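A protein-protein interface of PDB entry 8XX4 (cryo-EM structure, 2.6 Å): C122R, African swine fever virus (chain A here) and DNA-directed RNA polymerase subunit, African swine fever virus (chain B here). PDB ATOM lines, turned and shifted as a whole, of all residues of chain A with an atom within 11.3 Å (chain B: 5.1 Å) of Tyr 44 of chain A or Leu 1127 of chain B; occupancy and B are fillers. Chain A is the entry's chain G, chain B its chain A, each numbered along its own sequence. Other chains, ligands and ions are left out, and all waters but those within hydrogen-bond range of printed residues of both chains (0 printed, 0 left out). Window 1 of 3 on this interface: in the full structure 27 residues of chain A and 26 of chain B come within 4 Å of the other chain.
Along chain B the printed residues that touch a printed residue of chain A span positions 1123 to 1255. Among the printed residues, 10 pairs touch across the chains.
O of Leu 1255 of chain B sits at hydrogen-bond distance from N of Glu 1123 of chain B (2.9 Å). The backbone carbonyl oxygen of Glu 1179 of chain B is in hydrogen-bond range of the backbone NH of Leu 1127 of chain B, at 2.6 Å. The backbone carbonyl oxygen of Gln 1128 of chain B sits at hydrogen-bond distance from the backbone NH of Glu 1179 of chain B, at 2.7 Å. O of Tyr 44 of chain A lies within hydrogen-bond range of OG1 of Thr 46 of chain A, 3.2 Å away.
The side-chain carboxylate (OE2) of Glu 1123 of chain B is in hydrogen-bond range of the side-chain hydroxyl (OH) of Tyr 44 of chain A, 3.1 Å away. The backbone NH of Tyr 44 of chain A is in hydrogen-bond range of the backbone carbonyl oxygen of Leu 1127 of chain B. The backbone carbonyl oxygen (O) of Trp 1129 of chain B lies within hydrogen-bond range of the backbone NH (N) of Lys 42 of chain A, 3.0 Å away. The indole nitrogen (NE1) of Trp 1129 of chain B lies within hydrogen-bond range of the side-chain hydroxyl (OH) of Tyr 44 of chain A (3.2 Å).
Printed residues of chain B within 4 Å of Lys 42 of chain A: Gln 1128 (3.3 Å) and Trp 1129 (3.0 Å). Printed residues of chain B within 4 Å of Val 43 of chain A: Gln 1128 (3.6 Å). Tyr 44 of chain A touches just these residues of chain B: Glu 1123 (3.1 Å), Ile 1126 (3.5 Å), Leu 1127 (3.0 Å), Trp 1129 (3.2 Å) and Leu 1255 (3.6 Å). His 45 of chain A touches none of the printed residues of chain B. Of chain A, only Tyr 44 comes within 4 Å of Glu 1123 of chain B. Printed residues of chain A within 4 Å of Ile 1126 of chain B: Tyr 44. Leu 1127 of chain B touches just one residue of chain A: Tyr 44 (3.0 Å). Printed residues of chain A within 4 Å of Trp 1129 of chain B: Ser 40 (3.9 Å), Ser 41 (3.3 Å), Lys 42 (3.0 Å) and Tyr 44 (3.2 Å). No residue of chain A comes within 4 Å of Glu 1179 of chain B. No residue of chain A comes within 4 Å of Leu 1180 of chain B. No residue of chain A comes within 4 Å of Asn 1181 of chain B. Of the printed residues of chain A, Leu 1255 of chain B touches Tyr 44. The nearest residue of chain A that does not touch Leu 1127 of chain B is Val 43 of chain A (4.1 Å). The nearest printed residue of chain B that does not touch Lys 42 of chain A is Leu 1127 of chain B (4.7 Å).
OG of Ser 40 of chain A touches CH2 of Trp 1129 of chain B (3.9 Å). Ser 41 of chain A touches Trp 1129 of chain B. O of Lys 42 of chain A touches CA of Gln 1128 of chain B (3.3 Å). CG2 of Val 43 of chain A touches CB of Gln 1128 of chain B, 3.6 Å away. CD1 of Tyr 44 of chain A touches O of Ile 1126 of chain B, at 3.5 Å. Leu 1255 of chain B touches Tyr 44 of chain A.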
ATOM      1  N   SER A  40     -12.983   1.956 -19.645  1.00  0.00           N
ATOM      2  CA  SER A  40     -14.328   1.428 -19.797  1.00  0.00           C
ATOM      3  C   SER A  40     -14.609   0.480 -18.645  1.00  0.00           C
ATOM      4  O   SER A  40     -13.696   0.027 -17.952  1.00  0.00           O
ATOM      5  CB  SER A  40     -14.502   0.715 -21.141  1.00  0.00           C
ATOM      6  OG  SER A  40     -15.848   0.328 -21.339  1.00  0.00           O
ATOM      7  N   SER A  41     -15.890   0.193 -18.445  1.00  0.00           N
ATOM      8  CA  SER A  41     -16.301  -0.711 -17.385  1.00  0.00           C
ATOM      9  C   SER A  41     -17.705  -1.207 -17.680  1.00  0.00           C
ATOM     10  O   SER A  41     -18.429  -0.636 -18.499  1.00  0.00           O
ATOM     11  CB  SER A  41     -16.244  -0.032 -16.014  1.00  0.00           C
ATOM     12  OG  SER A  41     -17.229   0.979 -15.904  1.00  0.00           O
ATOM     13  N   LYS A  42     -18.075  -2.288 -17.003  1.00  0.00           N
ATOM     14  CA  LYS A  42     -19.432  -2.806 -17.065  1.00  0.00           C
ATOM     15  C   LYS A  42     -19.729  -3.501 -15.749  1.00  0.00           C
ATOM     16  O   LYS A  42     -18.928  -4.316 -15.283  1.00  0.00           O
ATOM     17  CB  LYS A  42     -19.615  -3.772 -18.237  1.00  0.00           C
ATOM     18  CG  LYS A  42     -20.851  -4.642 -18.128  1.00  0.00           C
ATOM     19  CD  LYS A  42     -21.617  -4.673 -19.436  1.00  0.00           C
ATOM     20  CE  LYS A  42     -22.886  -5.502 -19.315  1.00  0.00           C
ATOM     21  NZ  LYS A  42     -24.069  -4.790 -19.876  1.00  0.00           N
ATOM     22  N   VAL A  43     -20.868  -3.172 -15.152  1.00  0.00           N
ATOM     23  CA  VAL A  43     -21.277  -3.728 -13.871  1.00  0.00           C
ATOM     24  C   VAL A  43     -22.556  -4.521 -14.093  1.00  0.00           C
ATOM     25  O   VAL A  43     -23.540  -3.989 -14.618  1.00  0.00           O
ATOM     26  CB  VAL A  43     -21.478  -2.628 -12.816  1.00  0.00           C
ATOM     27  CG1 VAL A  43     -22.252  -3.166 -11.646  1.00  0.00           C
ATOM     28  CG2 VAL A  43     -20.137  -2.077 -12.361  1.00  0.00           C
ATOM     29  N   TYR A  44     -22.537  -5.793 -13.699  1.00  0.00           N
ATOM     30  CA  TYR A  44     -23.623  -6.720 -13.997  1.00  0.00           C
ATOM     31  C   TYR A  44     -24.606  -6.738 -12.833  1.00  0.00           C
ATOM     32  O   TYR A  44     -24.262  -7.180 -11.732  1.00  0.00           O
ATOM     33  CB  TYR A  44     -23.073  -8.117 -14.273  1.00  0.00           C
ATOM     34  CG  TYR A  44     -22.186  -8.199 -15.494  1.00  0.00           C
ATOM     35  CD1 TYR A  44     -20.852  -7.824 -15.435  1.00  0.00           C
ATOM     36  CD2 TYR A  44     -22.684  -8.650 -16.708  1.00  0.00           C
ATOM     37  CE1 TYR A  44     -20.042  -7.896 -16.547  1.00  0.00           C
ATOM     38  CE2 TYR A  44     -21.880  -8.723 -17.826  1.00  0.00           C
ATOM     39  CZ  TYR A  44     -20.560  -8.345 -17.739  1.00  0.00           C
ATOM     40  OH  TYR A  44     -19.755  -8.417 -18.851  1.00  0.00           O
ATOM     41  N   HIS A  45     -25.826  -6.272 -13.092  1.00  0.00           N
ATOM     42  CA  HIS A  45     -26.952  -6.283 -12.152  1.00  0.00           C
ATOM     43  C   HIS A  45     -26.528  -5.878 -10.738  1.00  0.00           C
ATOM     44  O   HIS A  45     -26.622  -6.645  -9.781  1.00  0.00           O
ATOM     45  CB  HIS A  45     -27.663  -7.639 -12.146  1.00  0.00           C
ATOM     46  CG  HIS A  45     -26.754  -8.811 -11.950  1.00  0.00           C
ATOM     47  ND1 HIS A  45     -26.202  -9.510 -13.003  1.00  0.00           N
ATOM     48  CD2 HIS A  45     -26.302  -9.411 -10.823  1.00  0.00           C
ATOM     49  CE1 HIS A  45     -25.448 -10.487 -12.533  1.00  0.00           C
ATOM     50  NE2 HIS A  45     -25.490 -10.449 -11.214  1.00  0.00           N
ATOM     51  N   THR A  46     -26.054  -4.638 -10.626  1.00  0.00           N
ATOM     52  CA  THR A  46     -25.712  -4.050  -9.328  1.00  0.00           C
ATOM     53  C   THR A  46     -26.103  -2.576  -9.372  1.00  0.00           C
ATOM     54  O   THR A  46     -25.396  -1.757  -9.967  1.00  0.00           O
ATOM     55  CB  THR A  46     -24.232  -4.222  -9.005  1.00  0.00           C
ATOM     56  OG1 THR A  46     -23.894  -5.616  -9.013  1.00  0.00           O
ATOM     57  CG2 THR A  46     -23.917  -3.635  -7.637  1.00  0.00           C
ATOM     58  N   GLY A  47     -27.231  -2.246  -8.747  1.00  0.00           N
ATOM     59  CA  GLY A  47     -27.729  -0.885  -8.729  1.00  0.00           C
ATOM     60  C   GLY A  47     -28.836  -0.674  -9.739  1.00  0.00           C
ATOM     61  O   GLY A  47     -28.566  -0.466 -10.926  1.00  0.00           O
ATOM     62  N   GLU A  48     -30.080  -0.708  -9.284  1.00  0.00           N
ATOM     63  CA  GLU A  48     -31.229  -0.683 -10.185  1.00  0.00           C
ATOM     64  C   GLU A  48     -32.476  -0.402  -9.355  1.00  0.00           C
ATOM     65  O   GLU A  48     -32.392  -0.124  -8.152  1.00  0.00           O
ATOM     66  CB  GLU A  48     -31.345  -1.998 -10.956  1.00  0.00           C
ATOM     67  CG  GLU A  48     -31.599  -1.840 -12.435  1.00  0.00           C
ATOM     68  CD  GLU A  48     -32.207  -3.084 -13.039  1.00  0.00           C
ATOM     69  OE1 GLU A  48     -32.119  -4.156 -12.405  1.00  0.00           O
ATOM     70  OE2 GLU A  48     -32.772  -2.993 -14.149  1.00  0.00           O
ATOM     71  N   ASP A  51     -33.119   3.517  -8.333  1.00  0.00           N
ATOM     72  CA  ASP A  51     -32.506   4.628  -9.052  1.00  0.00           C
ATOM     73  C   ASP A  51     -33.333   5.032 -10.268  1.00  0.00           C
ATOM     74  O   ASP A  51     -33.531   6.224 -10.522  1.00  0.00           O
ATOM     75  CB  ASP A  51     -31.078   4.266  -9.464  1.00  0.00           C
ATOM     76  CG  ASP A  51     -31.026   3.121 -10.463  1.00  0.00           C
ATOM     77  OD1 ASP A  51     -32.036   2.402 -10.603  1.00  0.00           O
ATOM     78  OD2 ASP A  51     -29.973   2.946 -11.113  1.00  0.00           O
ATOM     79  N   GLN A  89     -37.429  -8.904 -11.045  1.00  0.00           N
ATOM     80  CA  GLN A  89     -37.271  -9.619  -9.789  1.00  0.00           C
ATOM     81  C   GLN A  89     -38.403  -9.338  -8.814  1.00  0.00           C
ATOM     82  O   GLN A  89     -38.396  -9.872  -7.703  1.00  0.00           O
ATOM     83  CB  GLN A  89     -35.924  -9.286  -9.150  1.00  0.00           C
ATOM     84  CG  GLN A  89     -35.600  -7.815  -9.095  1.00  0.00           C
ATOM     85  CD  GLN A  89     -34.175  -7.540  -9.520  1.00  0.00           C
ATOM     86  OE1 GLN A  89     -33.231  -7.792  -8.770  1.00  0.00           O
ATOM     87  NE2 GLN A  89     -34.010  -7.024 -10.734  1.00  0.00           N
ATOM     88  N   GLU B1123     -17.820 -14.410 -19.070  1.00  0.00           N
ATOM     89  CA  GLU B1123     -18.741 -13.338 -18.716  1.00  0.00           C
ATOM     90  C   GLU B1123     -19.751 -13.752 -17.656  1.00  0.00           C
ATOM     91  O   GLU B1123     -20.309 -12.883 -16.980  1.00  0.00           O
ATOM     92  CB  GLU B1123     -19.477 -12.856 -19.963  1.00  0.00           C
ATOM     93  CG  GLU B1123     -20.095 -11.480 -19.838  1.00  0.00           C
ATOM     94  CD  GLU B1123     -20.809 -11.051 -21.102  1.00  0.00           C
ATOM     95  OE1 GLU B1123     -21.296 -11.935 -21.837  1.00  0.00           O
ATOM     96  OE2 GLU B1123     -20.879  -9.833 -21.366  1.00  0.00           O
ATOM     97  N   LEU B1125     -19.169 -15.474 -14.914  1.00  0.00           N
ATOM     98  CA  LEU B1125     -18.576 -15.486 -13.585  1.00  0.00           C
ATOM     99  C   LEU B1125     -18.120 -14.102 -13.146  1.00  0.00           C
ATOM    100  O   LEU B1125     -17.529 -13.966 -12.069  1.00  0.00           O
ATOM    101  CB  LEU B1125     -17.402 -16.463 -13.540  1.00  0.00           C
ATOM    102  CG  LEU B1125     -17.594 -17.764 -14.316  1.00  0.00           C
ATOM    103  CD1 LEU B1125     -16.255 -18.369 -14.678  1.00  0.00           C
ATOM    104  CD2 LEU B1125     -18.411 -18.738 -13.497  1.00  0.00           C
ATOM    105  N   ILE B1126     -18.390 -13.075 -13.942  1.00  0.00           N
ATOM    106  CA  ILE B1126     -17.896 -11.729 -13.691  1.00  0.00           C
ATOM    107  C   ILE B1126     -19.001 -10.922 -13.030  1.00  0.00           C
ATOM    108  O   ILE B1126     -20.080 -10.741 -13.606  1.00  0.00           O
ATOM    109  CB  ILE B1126     -17.429 -11.055 -14.990  1.00  0.00           C
ATOM    110  CG1 ILE B1126     -16.161 -11.720 -15.518  1.00  0.00           C
ATOM    111  CG2 ILE B1126     -17.187  -9.584 -14.765  1.00  0.00           C
ATOM    112  CD1 ILE B1126     -15.239 -12.222 -14.444  1.00  0.00           C
ATOM    113  N   LEU B1127     -18.740 -10.441 -11.815  1.00  0.00           N
ATOM    114  CA  LEU B1127     -19.638  -9.471 -11.200  1.00  0.00           C
ATOM    115  C   LEU B1127     -19.527  -8.120 -11.894  1.00  0.00           C
ATOM    116  O   LEU B1127     -20.539  -7.482 -12.202  1.00  0.00           O
ATOM    117  CB  LEU B1127     -19.328  -9.343  -9.710  1.00  0.00           C
ATOM    118  CG  LEU B1127     -20.200 -10.111  -8.717  1.00  0.00           C
ATOM    119  CD1 LEU B1127     -19.684  -9.908  -7.308  1.00  0.00           C
ATOM    120  CD2 LEU B1127     -21.652  -9.682  -8.825  1.00  0.00           C
ATOM    121  N   GLN B1128     -18.299  -7.673 -12.148  1.00  0.00           N
ATOM    122  CA  GLN B1128     -18.041  -6.447 -12.889  1.00  0.00           C
ATOM    123  C   GLN B1128     -16.597  -6.462 -13.361  1.00  0.00           C
ATOM    124  O   GLN B1128     -15.747  -7.149 -12.790  1.00  0.00           O
ATOM    125  CB  GLN B1128     -18.320  -5.205 -12.038  1.00  0.00           C
ATOM    126  CG  GLN B1128     -17.210  -4.835 -11.072  1.00  0.00           C
ATOM    127  CD  GLN B1128     -17.740  -4.148  -9.831  1.00  0.00           C
ATOM    128  OE1 GLN B1128     -18.918  -4.266  -9.500  1.00  0.00           O
ATOM    129  NE2 GLN B1128     -16.873  -3.417  -9.142  1.00  0.00           N
ATOM    130  N   TRP B1129     -16.329  -5.704 -14.422  1.00  0.00           N
ATOM    131  CA  TRP B1129     -14.982  -5.592 -14.959  1.00  0.00           C
ATOM    132  C   TRP B1129     -14.681  -4.139 -15.287  1.00  0.00           C
ATOM    133  O   TRP B1129     -15.573  -3.370 -15.647  1.00  0.00           O
ATOM    134  CB  TRP B1129     -14.784  -6.463 -16.207  1.00  0.00           C
ATOM    135  CG  TRP B1129     -15.691  -6.139 -17.351  1.00  0.00           C
ATOM    136  CD1 TRP B1129     -16.875  -6.739 -17.649  1.00  0.00           C
ATOM    137  CD2 TRP B1129     -15.478  -5.147 -18.362  1.00  0.00           C
ATOM    138  NE1 TRP B1129     -17.417  -6.182 -18.778  1.00  0.00           N
ATOM    139  CE2 TRP B1129     -16.577  -5.201 -19.236  1.00  0.00           C
ATOM    140  CE3 TRP B1129     -14.466  -4.218 -18.611  1.00  0.00           C
ATOM    141  CZ2 TRP B1129     -16.694  -4.362 -20.337  1.00  0.00           C
ATOM    142  CZ3 TRP B1129     -14.585  -3.387 -19.705  1.00  0.00           C
ATOM    143  CH2 TRP B1129     -15.689  -3.464 -20.554  1.00  0.00           C
ATOM    144  N   GLU B1179     -14.054  -8.550 -11.269  1.00  0.00           N
ATOM    145  CA  GLU B1179     -14.579  -8.943  -9.970  1.00  0.00           C
ATOM    146  C   GLU B1179     -15.391 -10.216 -10.160  1.00  0.00           C
ATOM    147  O   GLU B1179     -16.331 -10.237 -10.960  1.00  0.00           O
ATOM    148  CB  GLU B1179     -15.439  -7.815  -9.403  1.00  0.00           C
ATOM    149  CG  GLU B1179     -16.425  -8.185  -8.312  1.00  0.00           C
ATOM    150  CD  GLU B1179     -16.380  -7.213  -7.161  1.00  0.00           C
ATOM    151  OE1 GLU B1179     -16.511  -7.649  -6.000  1.00  0.00           O
ATOM    152  OE2 GLU B1179     -16.212  -6.003  -7.415  1.00  0.00           O
ATOM    153  N   LEU B1180     -15.032 -11.270  -9.434  1.00  0.00           N
ATOM    154  CA  LEU B1180     -15.603 -12.586  -9.679  1.00  0.00           C
ATOM    155  C   LEU B1180     -16.807 -12.824  -8.777  1.00  0.00           C
ATOM    156  O   LEU B1180     -16.793 -12.481  -7.592  1.00  0.00           O
ATOM    157  CB  LEU B1180     -14.567 -13.689  -9.465  1.00  0.00           C
ATOM    158  CG  LEU B1180     -13.718 -14.105 -10.667  1.00  0.00           C
ATOM    159  CD1 LEU B1180     -14.433 -15.150 -11.495  1.00  0.00           C
ATOM    160  CD2 LEU B1180     -13.313 -12.916 -11.519  1.00  0.00           C
ATOM    161  N   ASN B1181     -17.850 -13.410  -9.352  1.00  0.00           N
ATOM    162  CA  ASN B1181     -19.060 -13.739  -8.612  1.00  0.00           C
ATOM    163  C   ASN B1181     -18.847 -15.045  -7.861  1.00  0.00           C
ATOM    164  O   ASN B1181     -18.918 -16.126  -8.451  1.00  0.00           O
ATOM    165  CB  ASN B1181     -20.243 -13.847  -9.565  1.00  0.00           C
ATOM    166  CG  ASN B1181     -21.564 -13.739  -8.858  1.00  0.00           C
ATOM    167  OD1 ASN B1181     -21.626 -13.719  -7.631  1.00  0.00           O
ATOM    168  ND2 ASN B1181     -22.639 -13.678  -9.629  1.00  0.00           N
ATOM    169  N   LEU B1255     -14.074 -11.929 -22.261  1.00  0.00           N
ATOM    170  CA  LEU B1255     -15.393 -12.182 -21.694  1.00  0.00           C
ATOM    171  C   LEU B1255     -16.099 -13.328 -22.403  1.00  0.00           C
ATOM    172  O   LEU B1255     -16.939 -14.005 -21.800  1.00  0.00           O
ATOM    173  CB  LEU B1255     -16.247 -10.919 -21.764  1.00  0.00           C
ATOM    174  CG  LEU B1255     -15.864  -9.790 -20.812  1.00  0.00           C
ATOM    175  CD1 LEU B1255     -16.818  -8.629 -20.989  1.00  0.00           C
ATOM    176  CD2 LEU B1255     -15.859 -10.274 -19.375  1.00  0.00           C
